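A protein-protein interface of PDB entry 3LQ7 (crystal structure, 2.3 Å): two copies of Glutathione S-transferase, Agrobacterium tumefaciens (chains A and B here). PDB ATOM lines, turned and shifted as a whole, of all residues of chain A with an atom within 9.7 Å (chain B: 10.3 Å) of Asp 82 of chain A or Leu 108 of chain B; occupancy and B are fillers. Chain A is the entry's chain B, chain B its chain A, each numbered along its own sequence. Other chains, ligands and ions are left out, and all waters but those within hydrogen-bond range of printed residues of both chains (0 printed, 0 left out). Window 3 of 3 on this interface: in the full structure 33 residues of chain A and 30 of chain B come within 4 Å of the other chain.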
ATOM      1  N   LYS A  16      -6.551 -31.550 -34.352  1.00  0.00           N
ATOM      2  CA  LYS A  16      -7.215 -30.224 -34.172  1.00  0.00           C
ATOM      3  C   LYS A  16      -6.289 -29.063 -34.557  1.00  0.00           C
ATOM      4  O   LYS A  16      -5.145 -29.004 -34.090  1.00  0.00           O
ATOM      5  CB  LYS A  16      -7.733 -30.072 -32.738  1.00  0.00           C
ATOM      6  CG  LYS A  16      -9.084 -30.731 -32.520  1.00  0.00           C
ATOM      7  CD  LYS A  16      -9.558 -30.594 -31.087  1.00  0.00           C
ATOM      8  CE  LYS A  16     -10.826 -31.404 -30.855  1.00  0.00           C
ATOM      9  NZ  LYS A  16     -11.149 -31.544 -29.408  1.00  0.00           N
ATOM     10  N   PRO A  17      -6.788 -28.132 -35.404  1.00  0.00           N
ATOM     11  CA  PRO A  17      -5.970 -27.092 -36.034  1.00  0.00           C
ATOM     12  C   PRO A  17      -5.337 -26.129 -35.035  1.00  0.00           C
ATOM     13  O   PRO A  17      -5.835 -25.980 -33.920  1.00  0.00           O
ATOM     14  CB  PRO A  17      -6.976 -26.345 -36.912  1.00  0.00           C
ATOM     15  CG  PRO A  17      -8.280 -26.555 -36.235  1.00  0.00           C
ATOM     16  CD  PRO A  17      -8.214 -27.963 -35.739  1.00  0.00           C
ATOM     17  N   ASN A  18      -4.243 -25.494 -35.447  1.00  0.00           N
ATOM     18  CA  ASN A  18      -3.525 -24.551 -34.602  1.00  0.00           C
ATOM     19  C   ASN A  18      -4.334 -23.291 -34.323  1.00  0.00           C
ATOM     20  O   ASN A  18      -4.962 -22.745 -35.229  1.00  0.00           O
ATOM     21  CB  ASN A  18      -2.169 -24.197 -35.213  1.00  0.00           C
ATOM     22  CG  ASN A  18      -1.214 -25.374 -35.233  1.00  0.00           C
ATOM     23  OD1 ASN A  18      -1.270 -26.255 -34.373  1.00  0.00           O
ATOM     24  ND2 ASN A  18      -0.328 -25.395 -36.224  1.00  0.00           N
ATOM     25  N   TYR A  78      -9.178 -15.893 -28.925  1.00  0.00           N
ATOM     26  CA  TYR A  78      -8.601 -17.197 -29.191  1.00  0.00           C
ATOM     27  C   TYR A  78      -9.549 -17.887 -30.158  1.00  0.00           C
ATOM     28  O   TYR A  78     -10.722 -18.068 -29.848  1.00  0.00           O
ATOM     29  CB  TYR A  78      -8.465 -17.978 -27.880  1.00  0.00           C
ATOM     30  CG  TYR A  78      -7.957 -19.407 -27.979  1.00  0.00           C
ATOM     31  CD1 TYR A  78      -8.839 -20.474 -28.193  1.00  0.00           C
ATOM     32  CD2 TYR A  78      -6.602 -19.700 -27.807  1.00  0.00           C
ATOM     33  CE1 TYR A  78      -8.382 -21.793 -28.264  1.00  0.00           C
ATOM     34  CE2 TYR A  78      -6.135 -21.015 -27.858  1.00  0.00           C
ATOM     35  CZ  TYR A  78      -7.030 -22.055 -28.096  1.00  0.00           C
ATOM     36  OH  TYR A  78      -6.572 -23.355 -28.168  1.00  0.00           O
ATOM     37  N   GLU A  79      -9.039 -18.248 -31.332  1.00  0.00           N
ATOM     38  CA  GLU A  79      -9.831 -18.939 -32.344  1.00  0.00           C
ATOM     39  C   GLU A  79      -9.216 -20.283 -32.697  1.00  0.00           C
ATOM     40  O   GLU A  79      -8.031 -20.364 -32.995  1.00  0.00           O
ATOM     41  CB  GLU A  79      -9.956 -18.094 -33.611  1.00  0.00           C
ATOM     42  CG  GLU A  79     -10.776 -16.825 -33.453  1.00  0.00           C
ATOM     43  CD  GLU A  79     -11.107 -16.182 -34.788  1.00  0.00           C
ATOM     44  OE1 GLU A  79     -10.278 -16.281 -35.722  1.00  0.00           O
ATOM     45  OE2 GLU A  79     -12.197 -15.580 -34.904  1.00  0.00           O
ATOM     46  N   GLN A  80     -10.036 -21.327 -32.667  1.00  0.00           N
ATOM     47  CA  GLN A  80      -9.610 -22.671 -33.027  1.00  0.00           C
ATOM     48  C   GLN A  80     -10.810 -23.443 -33.569  1.00  0.00           C
ATOM     49  O   GLN A  80     -11.641 -23.939 -32.800  1.00  0.00           O
ATOM     50  CB  GLN A  80      -9.003 -23.383 -31.814  1.00  0.00           C
ATOM     51  CG  GLN A  80      -8.426 -24.767 -32.096  1.00  0.00           C
ATOM     52  CD  GLN A  80      -8.100 -25.535 -30.826  1.00  0.00           C
ATOM     53  OE1 GLN A  80      -8.177 -24.998 -29.718  1.00  0.00           O
ATOM     54  NE2 GLN A  80      -7.739 -26.804 -30.982  1.00  0.00           N
ATOM     55  N   GLY A  81     -10.888 -23.538 -34.895  1.00  0.00           N
ATOM     56  CA  GLY A  81     -12.036 -24.135 -35.571  1.00  0.00           C
ATOM     57  C   GLY A  81     -13.257 -23.249 -35.426  1.00  0.00           C
ATOM     58  O   GLY A  81     -13.217 -22.064 -35.755  1.00  0.00           O
ATOM     59  N   ASP A  82     -14.336 -23.825 -34.906  1.00  0.00           N
ATOM     60  CA  ASP A  82     -15.587 -23.096 -34.698  1.00  0.00           C
ATOM     61  C   ASP A  82     -15.657 -22.428 -33.323  1.00  0.00           C
ATOM     62  O   ASP A  82     -16.627 -21.733 -33.012  1.00  0.00           O
ATOM     63  CB  ASP A  82     -16.787 -24.029 -34.902  1.00  0.00           C
ATOM     64  CG  ASP A  82     -16.872 -24.576 -36.326  1.00  0.00           C
ATOM     65  OD1 ASP A  82     -16.871 -23.770 -37.285  1.00  0.00           O
ATOM     66  OD2 ASP A  82     -16.946 -25.817 -36.482  1.00  0.00           O
ATOM     67  N   LEU A  83     -14.621 -22.641 -32.511  1.00  0.00           N
ATOM     68  CA  LEU A  83     -14.554 -22.084 -31.161  1.00  0.00           C
ATOM     69  C   LEU A  83     -13.847 -20.740 -31.120  1.00  0.00           C
ATOM     70  O   LEU A  83     -12.682 -20.627 -31.501  1.00  0.00           O
ATOM     71  CB  LEU A  83     -13.853 -23.054 -30.207  1.00  0.00           C
ATOM     72  CG  LEU A  83     -13.568 -22.543 -28.790  1.00  0.00           C
ATOM     73  CD1 LEU A  83     -14.854 -22.320 -28.001  1.00  0.00           C
ATOM     74  CD2 LEU A  83     -12.654 -23.504 -28.072  1.00  0.00           C
ATOM     75  N   ILE A  84     -14.565 -19.729 -30.645  1.00  0.00           N
ATOM     76  CA  ILE A  84     -13.981 -18.419 -30.376  1.00  0.00           C
ATOM     77  C   ILE A  84     -14.025 -18.227 -28.863  1.00  0.00           C
ATOM     78  O   ILE A  84     -15.021 -18.563 -28.216  1.00  0.00           O
ATOM     79  CB  ILE A  84     -14.710 -17.267 -31.137  1.00  0.00           C
ATOM     80  CG1 ILE A  84     -14.689 -17.503 -32.654  1.00  0.00           C
ATOM     81  CG2 ILE A  84     -14.070 -15.911 -30.851  1.00  0.00           C
ATOM     82  CD1 ILE A  84     -15.970 -18.102 -33.231  1.00  0.00           C
ATOM     83  N   LEU A  85     -12.931 -17.725 -28.298  1.00  0.00           N
ATOM     84  CA  LEU A  85     -12.836 -17.534 -26.860  1.00  0.00           C
ATOM     85  C   LEU A  85     -12.357 -16.150 -26.469  1.00  0.00           C
ATOM     86  O   LEU A  85     -11.510 -15.537 -27.131  1.00  0.00           O
ATOM     87  CB  LEU A  85     -11.930 -18.589 -26.220  1.00  0.00           C
ATOM     88  CG  LEU A  85     -12.474 -20.006 -26.017  1.00  0.00           C
ATOM     89  CD1 LEU A  85     -11.378 -20.918 -25.498  1.00  0.00           C
ATOM     90  CD2 LEU A  85     -13.655 -20.027 -25.066  1.00  0.00           C
ATOM     91  N   PHE A  86     -12.931 -15.667 -25.378  1.00  0.00           N
ATOM     92  CA  PHE A  86     -12.463 -14.467 -24.721  1.00  0.00           C
ATOM     93  C   PHE A  86     -12.208 -14.798 -23.256  1.00  0.00           C
ATOM     94  O   PHE A  86     -12.527 -15.908 -22.808  1.00  0.00           O
ATOM     95  CB  PHE A  86     -13.446 -13.300 -24.903  1.00  0.00           C
ATOM     96  CG  PHE A  86     -14.818 -13.543 -24.335  1.00  0.00           C
ATOM     97  CD1 PHE A  86     -15.226 -12.876 -23.186  1.00  0.00           C
ATOM     98  CD2 PHE A  86     -15.720 -14.401 -24.968  1.00  0.00           C
ATOM     99  CE1 PHE A  86     -16.502 -13.082 -22.656  1.00  0.00           C
ATOM    100  CE2 PHE A  86     -16.988 -14.613 -24.446  1.00  0.00           C
ATOM    101  CZ  PHE A  86     -17.379 -13.952 -23.291  1.00  0.00           C
ATOM    102  N   HIS A  94      -8.922 -23.632 -21.145  1.00  0.00           N
ATOM    103  CA  HIS A  94      -9.132 -24.469 -22.320  1.00  0.00           C
ATOM    104  C   HIS A  94      -7.849 -25.110 -22.847  1.00  0.00           C
ATOM    105  O   HIS A  94      -7.836 -26.294 -23.200  1.00  0.00           O
ATOM    106  CB  HIS A  94      -9.790 -23.652 -23.430  1.00  0.00           C
ATOM    107  CG  HIS A  94      -9.992 -24.423 -24.696  1.00  0.00           C
ATOM    108  ND1 HIS A  94     -10.805 -25.536 -24.765  1.00  0.00           N
ATOM    109  CD2 HIS A  94      -9.478 -24.254 -25.936  1.00  0.00           C
ATOM    110  CE1 HIS A  94     -10.789 -26.012 -25.997  1.00  0.00           C
ATOM    111  NE2 HIS A  94      -9.990 -25.253 -26.726  1.00  0.00           N
ATOM    112  N   GLN A  97      -6.795 -27.840 -20.157  1.00  0.00           N
ATOM    113  CA  GLN A  97      -7.594 -29.051 -19.929  1.00  0.00           C
ATOM    114  C   GLN A  97      -7.562 -30.070 -21.070  1.00  0.00           C
ATOM    115  O   GLN A  97      -7.947 -31.229 -20.883  1.00  0.00           O
ATOM    116  CB  GLN A  97      -9.030 -28.725 -19.507  1.00  0.00           C
ATOM    117  CG  GLN A  97      -9.817 -27.854 -20.461  1.00  0.00           C
ATOM    118  CD  GLN A  97     -11.037 -27.254 -19.795  1.00  0.00           C
ATOM    119  OE1 GLN A  97     -11.410 -27.644 -18.685  1.00  0.00           O
ATOM    120  NE2 GLN A  97     -11.669 -26.300 -20.469  1.00  0.00           N
ATOM    121  N   HIS A  98      -7.081 -29.641 -22.233  1.00  0.00           N
ATOM    122  CA  HIS A  98      -7.025 -30.504 -23.409  1.00  0.00           C
ATOM    123  C   HIS A  98      -5.602 -30.906 -23.800  1.00  0.00           C
ATOM    124  O   HIS A  98      -5.410 -31.728 -24.695  1.00  0.00           O
ATOM    125  CB  HIS A  98      -7.775 -29.864 -24.578  1.00  0.00           C
ATOM    126  CG  HIS A  98      -9.242 -29.709 -24.328  1.00  0.00           C
ATOM    127  ND1 HIS A  98      -9.813 -28.509 -23.960  1.00  0.00           N
ATOM    128  CD2 HIS A  98     -10.251 -30.612 -24.364  1.00  0.00           C
ATOM    129  CE1 HIS A  98     -11.113 -28.676 -23.795  1.00  0.00           C
ATOM    130  NE2 HIS A  98     -11.405 -29.943 -24.034  1.00  0.00           N
ATOM    131  N   LEU B 103     -23.683 -27.051 -16.979  1.00  0.00           N
ATOM    132  CA  LEU B 103     -22.748 -26.939 -18.102  1.00  0.00           C
ATOM    133  C   LEU B 103     -23.202 -27.768 -19.306  1.00  0.00           C
ATOM    134  O   LEU B 103     -23.699 -28.885 -19.133  1.00  0.00           O
ATOM    135  CB  LEU B 103     -21.350 -27.391 -17.690  1.00  0.00           C
ATOM    136  CG  LEU B 103     -20.531 -26.569 -16.703  1.00  0.00           C
ATOM    137  CD1 LEU B 103     -19.337 -27.398 -16.294  1.00  0.00           C
ATOM    138  CD2 LEU B 103     -20.091 -25.235 -17.286  1.00  0.00           C
ATOM    139  N   PRO B 104     -23.028 -27.229 -20.528  1.00  0.00           N
ATOM    140  CA  PRO B 104     -23.308 -27.989 -21.752  1.00  0.00           C
ATOM    141  C   PRO B 104     -22.383 -29.200 -21.946  1.00  0.00           C
ATOM    142  O   PRO B 104     -21.227 -29.169 -21.505  1.00  0.00           O
ATOM    143  CB  PRO B 104     -23.044 -26.971 -22.862  1.00  0.00           C
ATOM    144  CG  PRO B 104     -23.130 -25.642 -22.211  1.00  0.00           C
ATOM    145  CD  PRO B 104     -22.651 -25.834 -20.822  1.00  0.00           C
ATOM    146  N   GLU B 105     -22.901 -30.247 -22.598  1.00  0.00           N
ATOM    147  CA  GLU B 105     -22.108 -31.433 -22.978  1.00  0.00           C
ATOM    148  C   GLU B 105     -21.038 -31.146 -24.034  1.00  0.00           C
ATOM    149  O   GLU B 105     -19.898 -31.595 -23.901  1.00  0.00           O
ATOM    150  CB  GLU B 105     -23.010 -32.566 -23.480  1.00  0.00           C
ATOM    151  CG  GLU B 105     -23.183 -33.720 -22.504  1.00  0.00           C
ATOM    152  CD  GLU B 105     -24.356 -33.541 -21.554  1.00  0.00           C
ATOM    153  OE1 GLU B 105     -24.596 -34.457 -20.739  1.00  0.00           O
ATOM    154  OE2 GLU B 105     -25.042 -32.496 -21.619  1.00  0.00           O
ATOM    155  N   ASP B 106     -21.418 -30.416 -25.084  1.00  0.00           N
ATOM    156  CA  ASP B 106     -20.499 -30.064 -26.165  1.00  0.00           C
ATOM    157  C   ASP B 106     -19.394 -29.155 -25.644  1.00  0.00           C
ATOM    158  O   ASP B 106     -19.663 -28.174 -24.949  1.00  0.00           O
ATOM    159  CB  ASP B 106     -21.257 -29.407 -27.325  1.00  0.00           C
ATOM    160  CG  ASP B 106     -20.336 -28.818 -28.390  1.00  0.00           C
ATOM    161  OD1 ASP B 106     -19.316 -29.450 -28.743  1.00  0.00           O
ATOM    162  OD2 ASP B 106     -20.650 -27.720 -28.894  1.00  0.00           O
ATOM    163  N   GLN B 107     -18.156 -29.503 -25.991  1.00  0.00           N
ATOM    164  CA  GLN B 107     -16.967 -28.824 -25.481  1.00  0.00           C
ATOM    165  C   GLN B 107     -16.744 -27.432 -26.074  1.00  0.00           C
ATOM    166  O   GLN B 107     -16.097 -26.592 -25.445  1.00  0.00           O
ATOM    167  CB  GLN B 107     -15.726 -29.701 -25.664  1.00  0.00           C
ATOM    168  CG  GLN B 107     -15.693 -30.912 -24.733  1.00  0.00           C
ATOM    169  CD  GLN B 107     -14.350 -31.622 -24.721  1.00  0.00           C
ATOM    170  OE1 GLN B 107     -13.773 -31.914 -25.770  1.00  0.00           O
ATOM    171  NE2 GLN B 107     -13.849 -31.914 -23.525  1.00  0.00           N
ATOM    172  N   LEU B 108     -17.273 -27.200 -27.276  1.00  0.00           N
ATOM    173  CA  LEU B 108     -17.289 -25.869 -27.892  1.00  0.00           C
ATOM    174  C   LEU B 108     -18.199 -24.940 -27.089  1.00  0.00           C
ATOM    175  O   LEU B 108     -17.861 -23.778 -26.842  1.00  0.00           O
ATOM    176  CB  LEU B 108     -17.793 -25.945 -29.336  1.00  0.00           C
ATOM    177  CG  LEU B 108     -16.962 -26.673 -30.398  1.00  0.00           C
ATOM    178  CD1 LEU B 108     -17.843 -27.588 -31.245  1.00  0.00           C
ATOM    179  CD2 LEU B 108     -16.205 -25.688 -31.273  1.00  0.00           C
ATOM    180  N   ARG B 109     -19.353 -25.478 -26.694  1.00  0.00           N
ATOM    181  CA  ARG B 109     -20.339 -24.770 -25.880  1.00  0.00           C
ATOM    182  C   ARG B 109     -19.857 -24.605 -24.432  1.00  0.00           C
ATOM    183  O   ARG B 109     -20.080 -23.562 -23.817  1.00  0.00           O
ATOM    184  CB  ARG B 109     -21.692 -25.503 -25.927  1.00  0.00           C
ATOM    185  CG  ARG B 109     -22.561 -25.185 -27.152  1.00  0.00           C
ATOM    186  CD  ARG B 109     -23.442 -26.366 -27.598  1.00  0.00           C
ATOM    187  NE  ARG B 109     -24.685 -26.509 -26.836  1.00  0.00           N
ATOM    188  CZ  ARG B 109     -25.047 -27.595 -26.148  1.00  0.00           C
ATOM    189  NH1 ARG B 109     -24.270 -28.670 -26.107  1.00  0.00           N
ATOM    190  NH2 ARG B 109     -26.202 -27.610 -25.498  1.00  0.00           N
ATOM    191  N   ARG B 110     -19.184 -25.631 -23.913  1.00  0.00           N
ATOM    192  CA  ARG B 110     -18.713 -25.651 -22.525  1.00  0.00           C
ATOM    193  C   ARG B 110     -17.582 -24.645 -22.279  1.00  0.00           C
ATOM    194  O   ARG B 110     -17.548 -23.995 -21.225  1.00  0.00           O
ATOM    195  CB  ARG B 110     -18.286 -27.070 -22.119  1.00  0.00           C
ATOM    196  CG  ARG B 110     -17.917 -27.246 -20.648  1.00  0.00           C
ATOM    197  CD  ARG B 110     -17.453 -28.664 -20.363  1.00  0.00           C
ATOM    198  NE  ARG B 110     -18.518 -29.497 -19.806  1.00  0.00           N
ATOM    199  CZ  ARG B 110     -18.475 -30.076 -18.606  1.00  0.00           C
ATOM    200  NH1 ARG B 110     -19.494 -30.815 -18.186  1.00  0.00           N
ATOM    201  NH2 ARG B 110     -17.413 -29.928 -17.821  1.00  0.00           N
ATOM    202  N   ALA B 111     -16.681 -24.512 -23.256  1.00  0.00           N
ATOM    203  CA  ALA B 111     -15.561 -23.573 -23.171  1.00  0.00           C
ATOM    204  C   ALA B 111     -16.029 -22.120 -23.167  1.00  0.00           C
ATOM    205  O   ALA B 111     -15.436 -21.281 -22.499  1.00  0.00           O
ATOM    206  CB  ALA B 111     -14.566 -23.808 -24.301  1.00  0.00           C
ATOM    207  N   ARG B 112     -17.091 -21.843 -23.919  1.00  0.00           N
ATOM    208  CA  ARG B 112     -17.689 -20.513 -23.984  1.00  0.00           C
ATOM    209  C   ARG B 112     -18.436 -20.154 -22.697  1.00  0.00           C
ATOM    210  O   ARG B 112     -18.495 -18.986 -22.316  1.00  0.00           O
ATOM    211  CB  ARG B 112     -18.633 -20.405 -25.183  1.00  0.00           C
ATOM    212  CG  ARG B 112     -17.920 -20.210 -26.500  1.00  0.00           C
ATOM    213  CD  ARG B 112     -18.797 -19.473 -27.484  1.00  0.00           C
ATOM    214  NE  ARG B 112     -18.089 -18.312 -28.019  1.00  0.00           N
ATOM    215  CZ  ARG B 112     -18.287 -17.058 -27.622  1.00  0.00           C
ATOM    216  NH1 ARG B 112     -19.192 -16.776 -26.690  1.00  0.00           N
ATOM    217  NH2 ARG B 112     -17.582 -16.076 -28.167  1.00  0.00           N
ATOM    218  N   THR B 113     -19.006 -21.165 -22.046  1.00  0.00           N
ATOM    219  CA  THR B 113     -19.642 -20.999 -20.746  1.00  0.00           C
ATOM    220  C   THR B 113     -18.623 -20.557 -19.690  1.00  0.00           C
ATOM    221  O   THR B 113     -18.863 -19.585 -18.965  1.00  0.00           O
ATOM    222  CB  THR B 113     -20.336 -22.292 -20.293  1.00  0.00           C
ATOM    223  OG1 THR B 113     -21.174 -22.777 -21.353  1.00  0.00           O
ATOM    224  CG2 THR B 113     -21.180 -22.038 -19.050  1.00  0.00           C
ATOM    225  N   VAL B 114     -17.492 -21.262 -19.641  1.00  0.00           N
ATOM    226  CA  VAL B 114     -16.355 -20.932 -18.768  1.00  0.00           C
ATOM    227  C   VAL B 114     -15.878 -19.489 -18.992  1.00  0.00           C
ATOM    228  O   VAL B 114     -15.544 -18.787 -18.028  1.00  0.00           O
ATOM    229  CB  VAL B 114     -15.192 -21.970 -18.928  1.00  0.00           C
ATOM    230  CG1 VAL B 114     -13.925 -21.552 -18.176  1.00  0.00           C
ATOM    231  CG2 VAL B 114     -15.638 -23.334 -18.439  1.00  0.00           C
ATOM    232  N   ALA B 115     -15.887 -19.051 -20.255  1.00  0.00           N
ATOM    233  CA  ALA B 115     -15.550 -17.673 -20.622  1.00  0.00           C
ATOM    234  C   ALA B 115     -16.467 -16.664 -19.954  1.00  0.00           C
ATOM    235  O   ALA B 115     -15.997 -15.656 -19.426  1.00  0.00           O
ATOM    236  CB  ALA B 115     -15.553 -17.489 -22.144  1.00  0.00           C
ATOM    237  N   TRP B 116     -17.765 -16.956 -19.956  1.00  0.00           N
ATOM    238  CA  TRP B 116     -18.746 -16.108 -19.290  1.00  0.00           C
ATOM    239  C   TRP B 116     -18.636 -16.129 -17.762  1.00  0.00           C
ATOM    240  O   TRP B 116     -18.889 -15.109 -17.109  1.00  0.00           O
ATOM    241  CB  TRP B 116     -20.166 -16.400 -19.790  1.00  0.00           C
ATOM    242  CG  TRP B 116     -20.466 -15.748 -21.119  1.00  0.00           C
ATOM    243  CD1 TRP B 116     -20.690 -16.374 -22.311  1.00  0.00           C
ATOM    244  CD2 TRP B 116     -20.559 -14.337 -21.386  1.00  0.00           C
ATOM    245  NE1 TRP B 116     -20.929 -15.444 -23.300  1.00  0.00           N
ATOM    246  CE2 TRP B 116     -20.850 -14.189 -22.756  1.00  0.00           C
ATOM    247  CE3 TRP B 116     -20.430 -13.187 -20.597  1.00  0.00           C
ATOM    248  CZ2 TRP B 116     -20.997 -12.935 -23.358  1.00  0.00           C
ATOM    249  CZ3 TRP B 116     -20.595 -11.940 -21.196  1.00  0.00           C
ATOM    250  CH2 TRP B 116     -20.873 -11.826 -22.562  1.00  0.00           C
ATOM    251  N   GLU B 173     -25.755 -17.696 -23.105  1.00  0.00           N
ATOM    252  CA  GLU B 173     -25.332 -18.574 -24.192  1.00  0.00           C
ATOM    253  C   GLU B 173     -26.146 -19.869 -24.140  1.00  0.00           C
ATOM    254  O   GLU B 173     -25.774 -20.811 -23.443  1.00  0.00           O
ATOM    255  CB  GLU B 173     -23.835 -18.880 -24.052  1.00  0.00           C
ATOM    256  CG  GLU B 173     -23.140 -19.412 -25.306  1.00  0.00           C
ATOM    257  CD  GLU B 173     -22.352 -18.344 -26.055  1.00  0.00           C
ATOM    258  OE1 GLU B 173     -21.697 -17.491 -25.409  1.00  0.00           O
ATOM    259  OE2 GLU B 173     -22.379 -18.367 -27.303  1.00  0.00           O
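The guanidinium group (NE) of Arg 112 of chain B lies within hydrogen-bond range of the backbone carbonyl oxygen (O) of Ile 84 of chain A, at 3.1 Å.
NE2 of Gln 107 of chain B lies within hydrogen-bond range of NE2 of His 98 of chain A, 3.2 Å away.
The guanidinium group (NH1) of Arg 112 of chain B lies within salt-bridge range of the side-chain carboxylate (OE1) of Glu 173 of chain B (2.9 Å).
The indole nitrogen (NE1) of Trp 116 of chain B sits at hydrogen-bond distance from the side-chain carboxylate (OE1) of Glu 173 of chain B (3.0 Å).
N of Leu 108 of chain B sits close to OD1 of Asp 106 of chain B.
N of Leu 85 of chain A sits at hydrogen-bond distance from O of Tyr 78 of chain A.
O of His 94 of chain A sits at hydrogen-bond distance from ND1 of His 98 of chain A, 3.1 Å away.
Asp 82 of chain A touches Leu 108 of chain B.
Leu 83 of chain A touches Leu 108 of chain B.
CD1 of Leu 83 of chain A touches CB of Ala 111 of chain B, 3.998 Å away.
O of Ala 111 of chain B touches CD2 of Leu 85 of chain A, 3.4 Å away.
Arg 112 of chain B touches Phe 86 of chain A (NH1 to CE2, 3.8 Å).
O of Phe 86 of chain A touches CB of Ala 115 of chain B (3.5 Å).
Phe 86 of chain A touches Trp 116 of chain B (CZ to CE2, 3.5 Å).
Asp 82 of chain A touches just one residue of chain B: Leu 108.
Leu 108 of chain B touches two residues of chain A.
No residue of chain B comes within 4 Å of Gly 81 of chain A.
Printed residues of chain A within 4 Å of Trp 116 of chain B: Phe 86.
Printed residues of chain B within 4 Å of His 98 of chain A: Gln 107 (3.2 Å).
Printed residues of chain B within 4 Å of Ile 84 of chain A: Arg 112.
Printed residues of chain A within 4 Å of Ala 111 of chain B: Leu 83 (3.998 Å) and Leu 85 (3.4 Å).
Hydrophobic or aromatic side chains of chain A that line the printed part of chain B: Leu 83, Leu 85, Phe 86 and His 98.
Of the 15 printed residues of chain B, 6 touch a printed residue of chain A.
Hydrophobic or aromatic side chains of chain B that line the printed part of chain A: Leu 108, Ala 111, Ala 115 and Trp 116.
Among the printed residues, no Asp or Glu carboxylate lies within 4 Å of a Lys or Arg side-chain nitrogen of the other chain.
No position is printed for both chains.
Of the 9 pairs that touch across the chains among the printed residues, none has its exchanged pair printed and touching as well.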
